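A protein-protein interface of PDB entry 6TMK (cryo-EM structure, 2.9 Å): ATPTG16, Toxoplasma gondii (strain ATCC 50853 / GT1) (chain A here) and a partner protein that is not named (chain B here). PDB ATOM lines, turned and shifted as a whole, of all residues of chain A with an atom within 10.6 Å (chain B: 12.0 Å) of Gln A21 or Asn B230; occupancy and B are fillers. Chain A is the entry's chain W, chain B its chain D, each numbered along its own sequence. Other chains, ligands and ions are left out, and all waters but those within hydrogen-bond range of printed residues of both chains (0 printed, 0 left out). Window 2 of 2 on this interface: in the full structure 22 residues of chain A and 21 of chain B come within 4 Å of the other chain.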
ATOM      1  N   VAL A  14     -19.371  29.316  22.034  1.00  0.00           N
ATOM      2  CA  VAL A  14     -20.235  30.484  21.981  1.00  0.00           C
ATOM      3  C   VAL A  14     -21.234  30.406  23.128  1.00  0.00           C
ATOM      4  O   VAL A  14     -21.485  29.317  23.659  1.00  0.00           O
ATOM      5  CB  VAL A  14     -20.937  30.589  20.619  1.00  0.00           C
ATOM      6  CG1 VAL A  14     -19.911  30.600  19.519  1.00  0.00           C
ATOM      7  CG2 VAL A  14     -21.905  29.448  20.420  1.00  0.00           C
ATOM      8  N   PRO A  15     -21.808  31.529  23.552  1.00  0.00           N
ATOM      9  CA  PRO A  15     -22.754  31.488  24.674  1.00  0.00           C
ATOM     10  C   PRO A  15     -24.020  30.711  24.389  1.00  0.00           C
ATOM     11  O   PRO A  15     -24.721  30.336  25.336  1.00  0.00           O
ATOM     12  CB  PRO A  15     -23.046  32.972  24.937  1.00  0.00           C
ATOM     13  CG  PRO A  15     -22.550  33.692  23.757  1.00  0.00           C
ATOM     14  CD  PRO A  15     -21.434  32.905  23.208  1.00  0.00           C
ATOM     15  N   SER A  16     -24.347  30.460  23.123  1.00  0.00           N
ATOM     16  CA  SER A  16     -25.484  29.609  22.808  1.00  0.00           C
ATOM     17  C   SER A  16     -25.225  28.155  23.166  1.00  0.00           C
ATOM     18  O   SER A  16     -26.172  27.364  23.229  1.00  0.00           O
ATOM     19  CB  SER A  16     -25.811  29.717  21.320  1.00  0.00           C
ATOM     20  OG  SER A  16     -26.396  30.965  21.011  1.00  0.00           O
ATOM     21  N   ALA A  17     -23.968  27.790  23.405  1.00  0.00           N
ATOM     22  CA  ALA A  17     -23.622  26.416  23.727  1.00  0.00           C
ATOM     23  C   ALA A  17     -23.849  26.085  25.193  1.00  0.00           C
ATOM     24  O   ALA A  17     -24.155  24.934  25.521  1.00  0.00           O
ATOM     25  CB  ALA A  17     -22.169  26.159  23.352  1.00  0.00           C
ATOM     26  N   PHE A  18     -23.698  27.063  26.084  1.00  0.00           N
ATOM     27  CA  PHE A  18     -23.938  26.858  27.504  1.00  0.00           C
ATOM     28  C   PHE A  18     -25.414  26.779  27.863  1.00  0.00           C
ATOM     29  O   PHE A  18     -25.725  26.555  29.035  1.00  0.00           O
ATOM     30  CB  PHE A  18     -23.294  27.984  28.305  1.00  0.00           C
ATOM     31  CG  PHE A  18     -21.814  28.087  28.133  1.00  0.00           C
ATOM     32  CD1 PHE A  18     -20.959  27.419  28.977  1.00  0.00           C
ATOM     33  CD2 PHE A  18     -21.278  28.877  27.144  1.00  0.00           C
ATOM     34  CE1 PHE A  18     -19.603  27.523  28.823  1.00  0.00           C
ATOM     35  CE2 PHE A  18     -19.925  28.982  26.991  1.00  0.00           C
ATOM     36  CZ  PHE A  18     -19.086  28.307  27.831  1.00  0.00           C
ATOM     37  N   ALA A  19     -26.321  26.949  26.904  1.00  0.00           N
ATOM     38  CA  ALA A  19     -27.731  27.149  27.206  1.00  0.00           C
ATOM     39  C   ALA A  19     -28.531  25.863  27.354  1.00  0.00           C
ATOM     40  O   ALA A  19     -29.649  25.911  27.874  1.00  0.00           O
ATOM     41  CB  ALA A  19     -28.378  28.007  26.121  1.00  0.00           C
ATOM     42  N   SER A  20     -28.006  24.728  26.907  1.00  0.00           N
ATOM     43  CA  SER A  20     -28.652  23.430  27.099  1.00  0.00           C
ATOM     44  C   SER A  20     -29.998  23.336  26.390  1.00  0.00           C
ATOM     45  O   SER A  20     -30.804  22.455  26.698  1.00  0.00           O
ATOM     46  CB  SER A  20     -28.837  23.119  28.582  1.00  0.00           C
ATOM     47  OG  SER A  20     -29.333  21.810  28.765  1.00  0.00           O
ATOM     48  N   GLN A  21     -30.261  24.231  25.443  1.00  0.00           N
ATOM     49  CA  GLN A  21     -31.487  24.188  24.661  1.00  0.00           C
ATOM     50  C   GLN A  21     -31.208  24.733  23.270  1.00  0.00           C
ATOM     51  O   GLN A  21     -30.428  25.676  23.110  1.00  0.00           O
ATOM     52  CB  GLN A  21     -32.613  24.983  25.325  1.00  0.00           C
ATOM     53  CG  GLN A  21     -33.363  24.198  26.384  1.00  0.00           C
ATOM     54  CD  GLN A  21     -34.522  24.969  26.978  1.00  0.00           C
ATOM     55  OE1 GLN A  21     -34.911  26.019  26.468  1.00  0.00           O
ATOM     56  NE2 GLN A  21     -35.082  24.450  28.064  1.00  0.00           N
ATOM     57  N   GLN A  22     -31.837  24.128  22.271  1.00  0.00           N
ATOM     58  CA  GLN A  22     -31.624  24.515  20.885  1.00  0.00           C
ATOM     59  C   GLN A  22     -32.459  25.740  20.532  1.00  0.00           C
ATOM     60  O   GLN A  22     -32.181  26.846  20.995  1.00  0.00           O
ATOM     61  CB  GLN A  22     -31.979  23.361  19.953  1.00  0.00           C
ATOM     62  CG  GLN A  22     -31.492  23.538  18.527  1.00  0.00           C
ATOM     63  CD  GLN A  22     -31.155  22.220  17.857  1.00  0.00           C
ATOM     64  OE1 GLN A  22     -31.699  21.174  18.211  1.00  0.00           O
ATOM     65  NE2 GLN A  22     -30.268  22.267  16.870  1.00  0.00           N
ATOM     66  N   ARG A  33     -30.509  18.977  11.758  1.00  0.00           N
ATOM     67  CA  ARG A  33     -30.459  20.109  12.666  1.00  0.00           C
ATOM     68  C   ARG A  33     -29.098  20.792  12.606  1.00  0.00           C
ATOM     69  O   ARG A  33     -28.113  20.235  12.120  1.00  0.00           O
ATOM     70  CB  ARG A  33     -30.746  19.661  14.095  1.00  0.00           C
ATOM     71  CG  ARG A  33     -32.091  19.005  14.293  1.00  0.00           C
ATOM     72  CD  ARG A  33     -32.477  19.010  15.760  1.00  0.00           C
ATOM     73  NE  ARG A  33     -31.561  18.206  16.563  1.00  0.00           N
ATOM     74  CZ  ARG A  33     -31.789  16.951  16.946  1.00  0.00           C
ATOM     75  NH1 ARG A  33     -32.910  16.332  16.602  1.00  0.00           N
ATOM     76  NH2 ARG A  33     -30.886  16.307  17.671  1.00  0.00           N
ATOM     77  N   LYS A  34     -29.060  22.017  13.110  1.00  0.00           N
ATOM     78  CA  LYS A  34     -27.808  22.743  13.212  1.00  0.00           C
ATOM     79  C   LYS A  34     -26.975  22.210  14.374  1.00  0.00           C
ATOM     80  O   LYS A  34     -27.521  21.690  15.350  1.00  0.00           O
ATOM     81  CB  LYS A  34     -28.087  24.223  13.423  1.00  0.00           C
ATOM     82  CG  LYS A  34     -28.504  24.952  12.160  1.00  0.00           C
ATOM     83  CD  LYS A  34     -29.061  26.332  12.458  1.00  0.00           C
ATOM     84  CE  LYS A  34     -27.967  27.318  12.818  1.00  0.00           C
ATOM     85  NZ  LYS A  34     -27.248  27.756  11.595  1.00  0.00           N
ATOM     86  N   PRO A  35     -25.653  22.330  14.299  1.00  0.00           N
ATOM     87  CA  PRO A  35     -24.814  21.796  15.374  1.00  0.00           C
ATOM     88  C   PRO A  35     -25.020  22.535  16.685  1.00  0.00           C
ATOM     89  O   PRO A  35     -25.336  23.726  16.715  1.00  0.00           O
ATOM     90  CB  PRO A  35     -23.391  21.986  14.838  1.00  0.00           C
ATOM     91  CG  PRO A  35     -23.507  23.049  13.820  1.00  0.00           C
ATOM     92  CD  PRO A  35     -24.840  22.850  13.191  1.00  0.00           C
ATOM     93  N   LEU A  36     -24.827  21.804  17.779  1.00  0.00           N
ATOM     94  CA  LEU A  36     -25.033  22.349  19.113  1.00  0.00           C
ATOM     95  C   LEU A  36     -23.811  23.081  19.639  1.00  0.00           C
ATOM     96  O   LEU A  36     -23.951  24.073  20.363  1.00  0.00           O
ATOM     97  CB  LEU A  36     -25.411  21.230  20.080  1.00  0.00           C
ATOM     98  CG  LEU A  36     -26.548  20.321  19.632  1.00  0.00           C
ATOM     99  CD1 LEU A  36     -26.708  19.190  20.605  1.00  0.00           C
ATOM    100  CD2 LEU A  36     -27.832  21.095  19.502  1.00  0.00           C
ATOM    101  N   LEU A  37     -22.625  22.604  19.294  1.00  0.00           N
ATOM    102  CA  LEU A  37     -21.367  23.156  19.769  1.00  0.00           C
ATOM    103  C   LEU A  37     -20.685  23.928  18.652  1.00  0.00           C
ATOM    104  O   LEU A  37     -20.483  23.394  17.557  1.00  0.00           O
ATOM    105  CB  LEU A  37     -20.464  22.037  20.276  1.00  0.00           C
ATOM    106  CG  LEU A  37     -19.222  22.395  21.073  1.00  0.00           C
ATOM    107  CD1 LEU A  37     -19.574  23.220  22.273  1.00  0.00           C
ATOM    108  CD2 LEU A  37     -18.566  21.109  21.501  1.00  0.00           C
ATOM    109  N   LEU B 158     -26.437  36.171  13.449  1.00  0.00           N
ATOM    110  CA  LEU B 158     -26.003  35.136  14.378  1.00  0.00           C
ATOM    111  C   LEU B 158     -24.951  35.674  15.339  1.00  0.00           C
ATOM    112  O   LEU B 158     -25.022  35.442  16.551  1.00  0.00           O
ATOM    113  CB  LEU B 158     -25.480  33.940  13.598  1.00  0.00           C
ATOM    114  CG  LEU B 158     -25.173  32.667  14.365  1.00  0.00           C
ATOM    115  CD1 LEU B 158     -26.449  31.970  14.770  1.00  0.00           C
ATOM    116  CD2 LEU B 158     -24.352  31.784  13.481  1.00  0.00           C
ATOM    117  N   SER B 161     -26.532  37.700  18.069  1.00  0.00           N
ATOM    118  CA  SER B 161     -27.180  36.926  19.117  1.00  0.00           C
ATOM    119  C   SER B 161     -26.179  36.509  20.188  1.00  0.00           C
ATOM    120  O   SER B 161     -26.509  36.477  21.379  1.00  0.00           O
ATOM    121  CB  SER B 161     -27.864  35.704  18.512  1.00  0.00           C
ATOM    122  OG  SER B 161     -28.965  36.085  17.707  1.00  0.00           O
ATOM    123  N   GLU B 162     -24.955  36.181  19.782  1.00  0.00           N
ATOM    124  CA  GLU B 162     -23.902  35.768  20.696  1.00  0.00           C
ATOM    125  C   GLU B 162     -23.183  36.939  21.351  1.00  0.00           C
ATOM    126  O   GLU B 162     -22.288  36.711  22.171  1.00  0.00           O
ATOM    127  CB  GLU B 162     -22.884  34.889  19.968  1.00  0.00           C
ATOM    128  CG  GLU B 162     -23.474  33.805  19.098  1.00  0.00           C
ATOM    129  CD  GLU B 162     -24.446  32.911  19.840  1.00  0.00           C
ATOM    130  OE1 GLU B 162     -25.323  32.314  19.184  1.00  0.00           O
ATOM    131  OE2 GLU B 162     -24.331  32.800  21.077  1.00  0.00           O
ATOM    132  N   ARG B 178     -27.954  39.869  34.747  1.00  0.00           N
ATOM    133  CA  ARG B 178     -28.313  38.504  35.114  1.00  0.00           C
ATOM    134  C   ARG B 178     -28.038  38.246  36.587  1.00  0.00           C
ATOM    135  O   ARG B 178     -28.861  37.651  37.295  1.00  0.00           O
ATOM    136  CB  ARG B 178     -27.541  37.516  34.260  1.00  0.00           C
ATOM    137  CG  ARG B 178     -28.034  37.370  32.875  1.00  0.00           C
ATOM    138  CD  ARG B 178     -27.533  36.084  32.311  1.00  0.00           C
ATOM    139  NE  ARG B 178     -26.076  36.067  32.239  1.00  0.00           N
ATOM    140  CZ  ARG B 178     -25.371  36.508  31.203  1.00  0.00           C
ATOM    141  NH1 ARG B 178     -25.974  37.017  30.140  1.00  0.00           N
ATOM    142  NH2 ARG B 178     -24.052  36.444  31.239  1.00  0.00           N
ATOM    143  N   HIS B 182     -30.972  37.259  39.338  1.00  0.00           N
ATOM    144  CA  HIS B 182     -30.867  35.998  40.058  1.00  0.00           C
ATOM    145  C   HIS B 182     -30.817  36.231  41.565  1.00  0.00           C
ATOM    146  O   HIS B 182     -31.500  35.547  42.337  1.00  0.00           O
ATOM    147  CB  HIS B 182     -29.628  35.254  39.570  1.00  0.00           C
ATOM    148  CG  HIS B 182     -29.598  33.805  39.929  1.00  0.00           C
ATOM    149  ND1 HIS B 182     -28.470  33.031  39.772  1.00  0.00           N
ATOM    150  CD2 HIS B 182     -30.550  32.985  40.428  1.00  0.00           C
ATOM    151  CE1 HIS B 182     -28.727  31.799  40.166  1.00  0.00           C
ATOM    152  NE2 HIS B 182     -29.982  31.745  40.568  1.00  0.00           N
ATOM    153  N   HIS B 212     -38.251  25.478  43.905  1.00  0.00           N
ATOM    154  CA  HIS B 212     -39.372  26.252  43.394  1.00  0.00           C
ATOM    155  C   HIS B 212     -39.037  27.052  42.145  1.00  0.00           C
ATOM    156  O   HIS B 212     -39.955  27.444  41.417  1.00  0.00           O
ATOM    157  CB  HIS B 212     -39.890  27.199  44.481  1.00  0.00           C
ATOM    158  CG  HIS B 212     -40.896  26.571  45.395  1.00  0.00           C
ATOM    159  ND1 HIS B 212     -40.596  25.504  46.213  1.00  0.00           N
ATOM    160  CD2 HIS B 212     -42.193  26.874  45.634  1.00  0.00           C
ATOM    161  CE1 HIS B 212     -41.668  25.167  46.906  1.00  0.00           C
ATOM    162  NE2 HIS B 212     -42.652  25.984  46.574  1.00  0.00           N
ATOM    163  N   GLY B 213     -37.762  27.302  41.881  1.00  0.00           N
ATOM    164  CA  GLY B 213     -37.363  27.998  40.677  1.00  0.00           C
ATOM    165  C   GLY B 213     -37.325  27.091  39.462  1.00  0.00           C
ATOM    166  O   GLY B 213     -37.213  25.871  39.586  1.00  0.00           O
ATOM    167  N   GLN B 229     -32.259  26.570  35.646  1.00  0.00           N
ATOM    168  CA  GLN B 229     -31.463  25.349  35.615  1.00  0.00           C
ATOM    169  C   GLN B 229     -31.271  24.835  34.198  1.00  0.00           C
ATOM    170  O   GLN B 229     -31.030  23.647  33.996  1.00  0.00           O
ATOM    171  CB  GLN B 229     -32.114  24.259  36.460  1.00  0.00           C
ATOM    172  CG  GLN B 229     -32.279  24.605  37.921  1.00  0.00           C
ATOM    173  CD  GLN B 229     -33.027  23.533  38.685  1.00  0.00           C
ATOM    174  OE1 GLN B 229     -33.851  22.817  38.119  1.00  0.00           O
ATOM    175  NE2 GLN B 229     -32.734  23.408  39.974  1.00  0.00           N
ATOM    176  N   ASN B 230     -31.378  25.724  33.211  1.00  0.00           N
ATOM    177  CA  ASN B 230     -31.245  25.288  31.825  1.00  0.00           C
ATOM    178  C   ASN B 230     -29.820  24.831  31.553  1.00  0.00           C
ATOM    179  O   ASN B 230     -29.570  23.652  31.284  1.00  0.00           O
ATOM    180  CB  ASN B 230     -31.646  26.427  30.888  1.00  0.00           C
ATOM    181  CG  ASN B 230     -32.008  25.944  29.506  1.00  0.00           C
ATOM    182  OD1 ASN B 230     -32.456  24.813  29.328  1.00  0.00           O
ATOM    183  ND2 ASN B 230     -31.822  26.807  28.515  1.00  0.00           N
ATOM    184  N   GLY B 231     -28.869  25.751  31.640  1.00  0.00           N
ATOM    185  CA  GLY B 231     -27.470  25.396  31.613  1.00  0.00           C
ATOM    186  C   GLY B 231     -26.731  26.206  32.651  1.00  0.00           C
ATOM    187  O   GLY B 231     -27.124  26.241  33.820  1.00  0.00           O
ATOM    188  N   ILE B 232     -25.664  26.872  32.234  1.00  0.00           N
ATOM    189  CA  ILE B 232     -24.974  27.826  33.092  1.00  0.00           C
ATOM    190  C   ILE B 232     -24.743  29.111  32.310  1.00  0.00           C
ATOM    191  O   ILE B 232     -24.898  29.129  31.082  1.00  0.00           O
ATOM    192  CB  ILE B 232     -23.654  27.261  33.631  1.00  0.00           C
ATOM    193  CG1 ILE B 232     -22.755  26.817  32.489  1.00  0.00           C
ATOM    194  CG2 ILE B 232     -23.919  26.114  34.564  1.00  0.00           C
ATOM    195  CD1 ILE B 232     -21.343  26.698  32.878  1.00  0.00           C
ATOM    196  N   PRO B 233     -24.373  30.203  32.976  1.00  0.00           N
ATOM    197  CA  PRO B 233     -23.883  31.361  32.247  1.00  0.00           C
ATOM    198  C   PRO B 233     -22.514  31.076  31.660  1.00  0.00           C
ATOM    199  O   PRO B 233     -21.768  30.227  32.176  1.00  0.00           O
ATOM    200  CB  PRO B 233     -23.816  32.457  33.324  1.00  0.00           C
ATOM    201  CG  PRO B 233     -24.654  31.987  34.408  1.00  0.00           C
ATOM    202  CD  PRO B 233     -24.655  30.517  34.381  1.00  0.00           C
ATOM    203  N   PRO B 234     -22.137  31.757  30.588  1.00  0.00           N
ATOM    204  CA  PRO B 234     -20.807  31.538  30.021  1.00  0.00           C
ATOM    205  C   PRO B 234     -19.715  31.997  30.966  1.00  0.00           C
ATOM    206  O   PRO B 234     -19.865  32.960  31.722  1.00  0.00           O
ATOM    207  CB  PRO B 234     -20.823  32.364  28.736  1.00  0.00           C
ATOM    208  CG  PRO B 234     -22.234  32.568  28.432  1.00  0.00           C
ATOM    209  CD  PRO B 234     -22.966  32.595  29.712  1.00  0.00           C
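The side-chain amide nitrogen (ND2) of Asn B230 lies within hydrogen-bond range of the backbone carbonyl oxygen (O) of Ala A19 (2.4 Å). The side-chain carboxylate of Glu B162 is in hydrogen-bond range of the side-chain hydroxyl of Ser A16 (2.5 Å). OG of Ser A20 lies close to O of Asn B230 (3.1 Å). OD1 of Asn B230 sits at hydrogen-bond distance from NE2 of Gln A21, at 2.9 Å. The backbone NH (N) of Ile B232 lies within hydrogen-bond range of the backbone carbonyl oxygen (O) of Phe A18 (3.2 Å).
Pro A15 touches Glu B162. Pro A15 touches Pro B234. O of Phe A18 touches CA of Gly B231, 3.3 Å away. Phe A18 touches Pro B234 (CD2 to CB, 3.9 Å). N of Gly B231 touches O of Ala A19 (3.8 Å).
Gln A21 touches just one residue of chain B: Asn B230. Asn B230 touches just these residues of chain A: Ala A19 (2.4 Å), Ser A20 (2.8 Å) and Gln A21 (2.9 Å). Printed residues of chain B within 4 Å of Ser A16: Glu B162 (2.5 Å). Of chain B, only Asn B230 (2.4 Å) and Gly B231 (3.8 Å) come within 4 Å of Ala A19. Of the printed residues of chain B, Ser A20 touches Asn B230. No residue of chain B comes within 4 Å of Gln A22. Printed residues of chain A within 4 Å of Gly B231: Phe A18 and Ala A19. Printed residues of chain A within 4 Å of Pro B234: Pro A15 and Phe A18. Of the printed residues of chain A, Ile B232 touches Phe A18 (3.2 Å). Printed residues of chain B within 4 Å of Phe A18: Gly B231 (3.3 Å), Ile B232 (3.2 Å) and Pro B234 (3.9 Å). Ser B161 touches none of the printed residues of chain A. Ala A17 touches none of the printed residues of chain B. The nearest residue of chain B that does not touch Gln A21 is Gly B231 (6.5 Å).
Printed residues of chain A that touch a printed residue of chain B: Pro A15, Ser A16, Phe A18, Ala A19, Ser A20 and Gln A21. Printed residues of chain B that touch a printed residue of chain A: Glu B162, Asn B230, Gly B231, Ile B232 and Pro B234. Hydrophobic or aromatic side chains of chain B within 4 Å of the printed part of chain A: Ile B232 and Pro B234. Among the printed residues, 10 pairs touch across the chains. Among the printed residues, no Asp or Glu carboxylate lies within 4 Å of a Lys or Arg side-chain nitrogen of the other chain.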
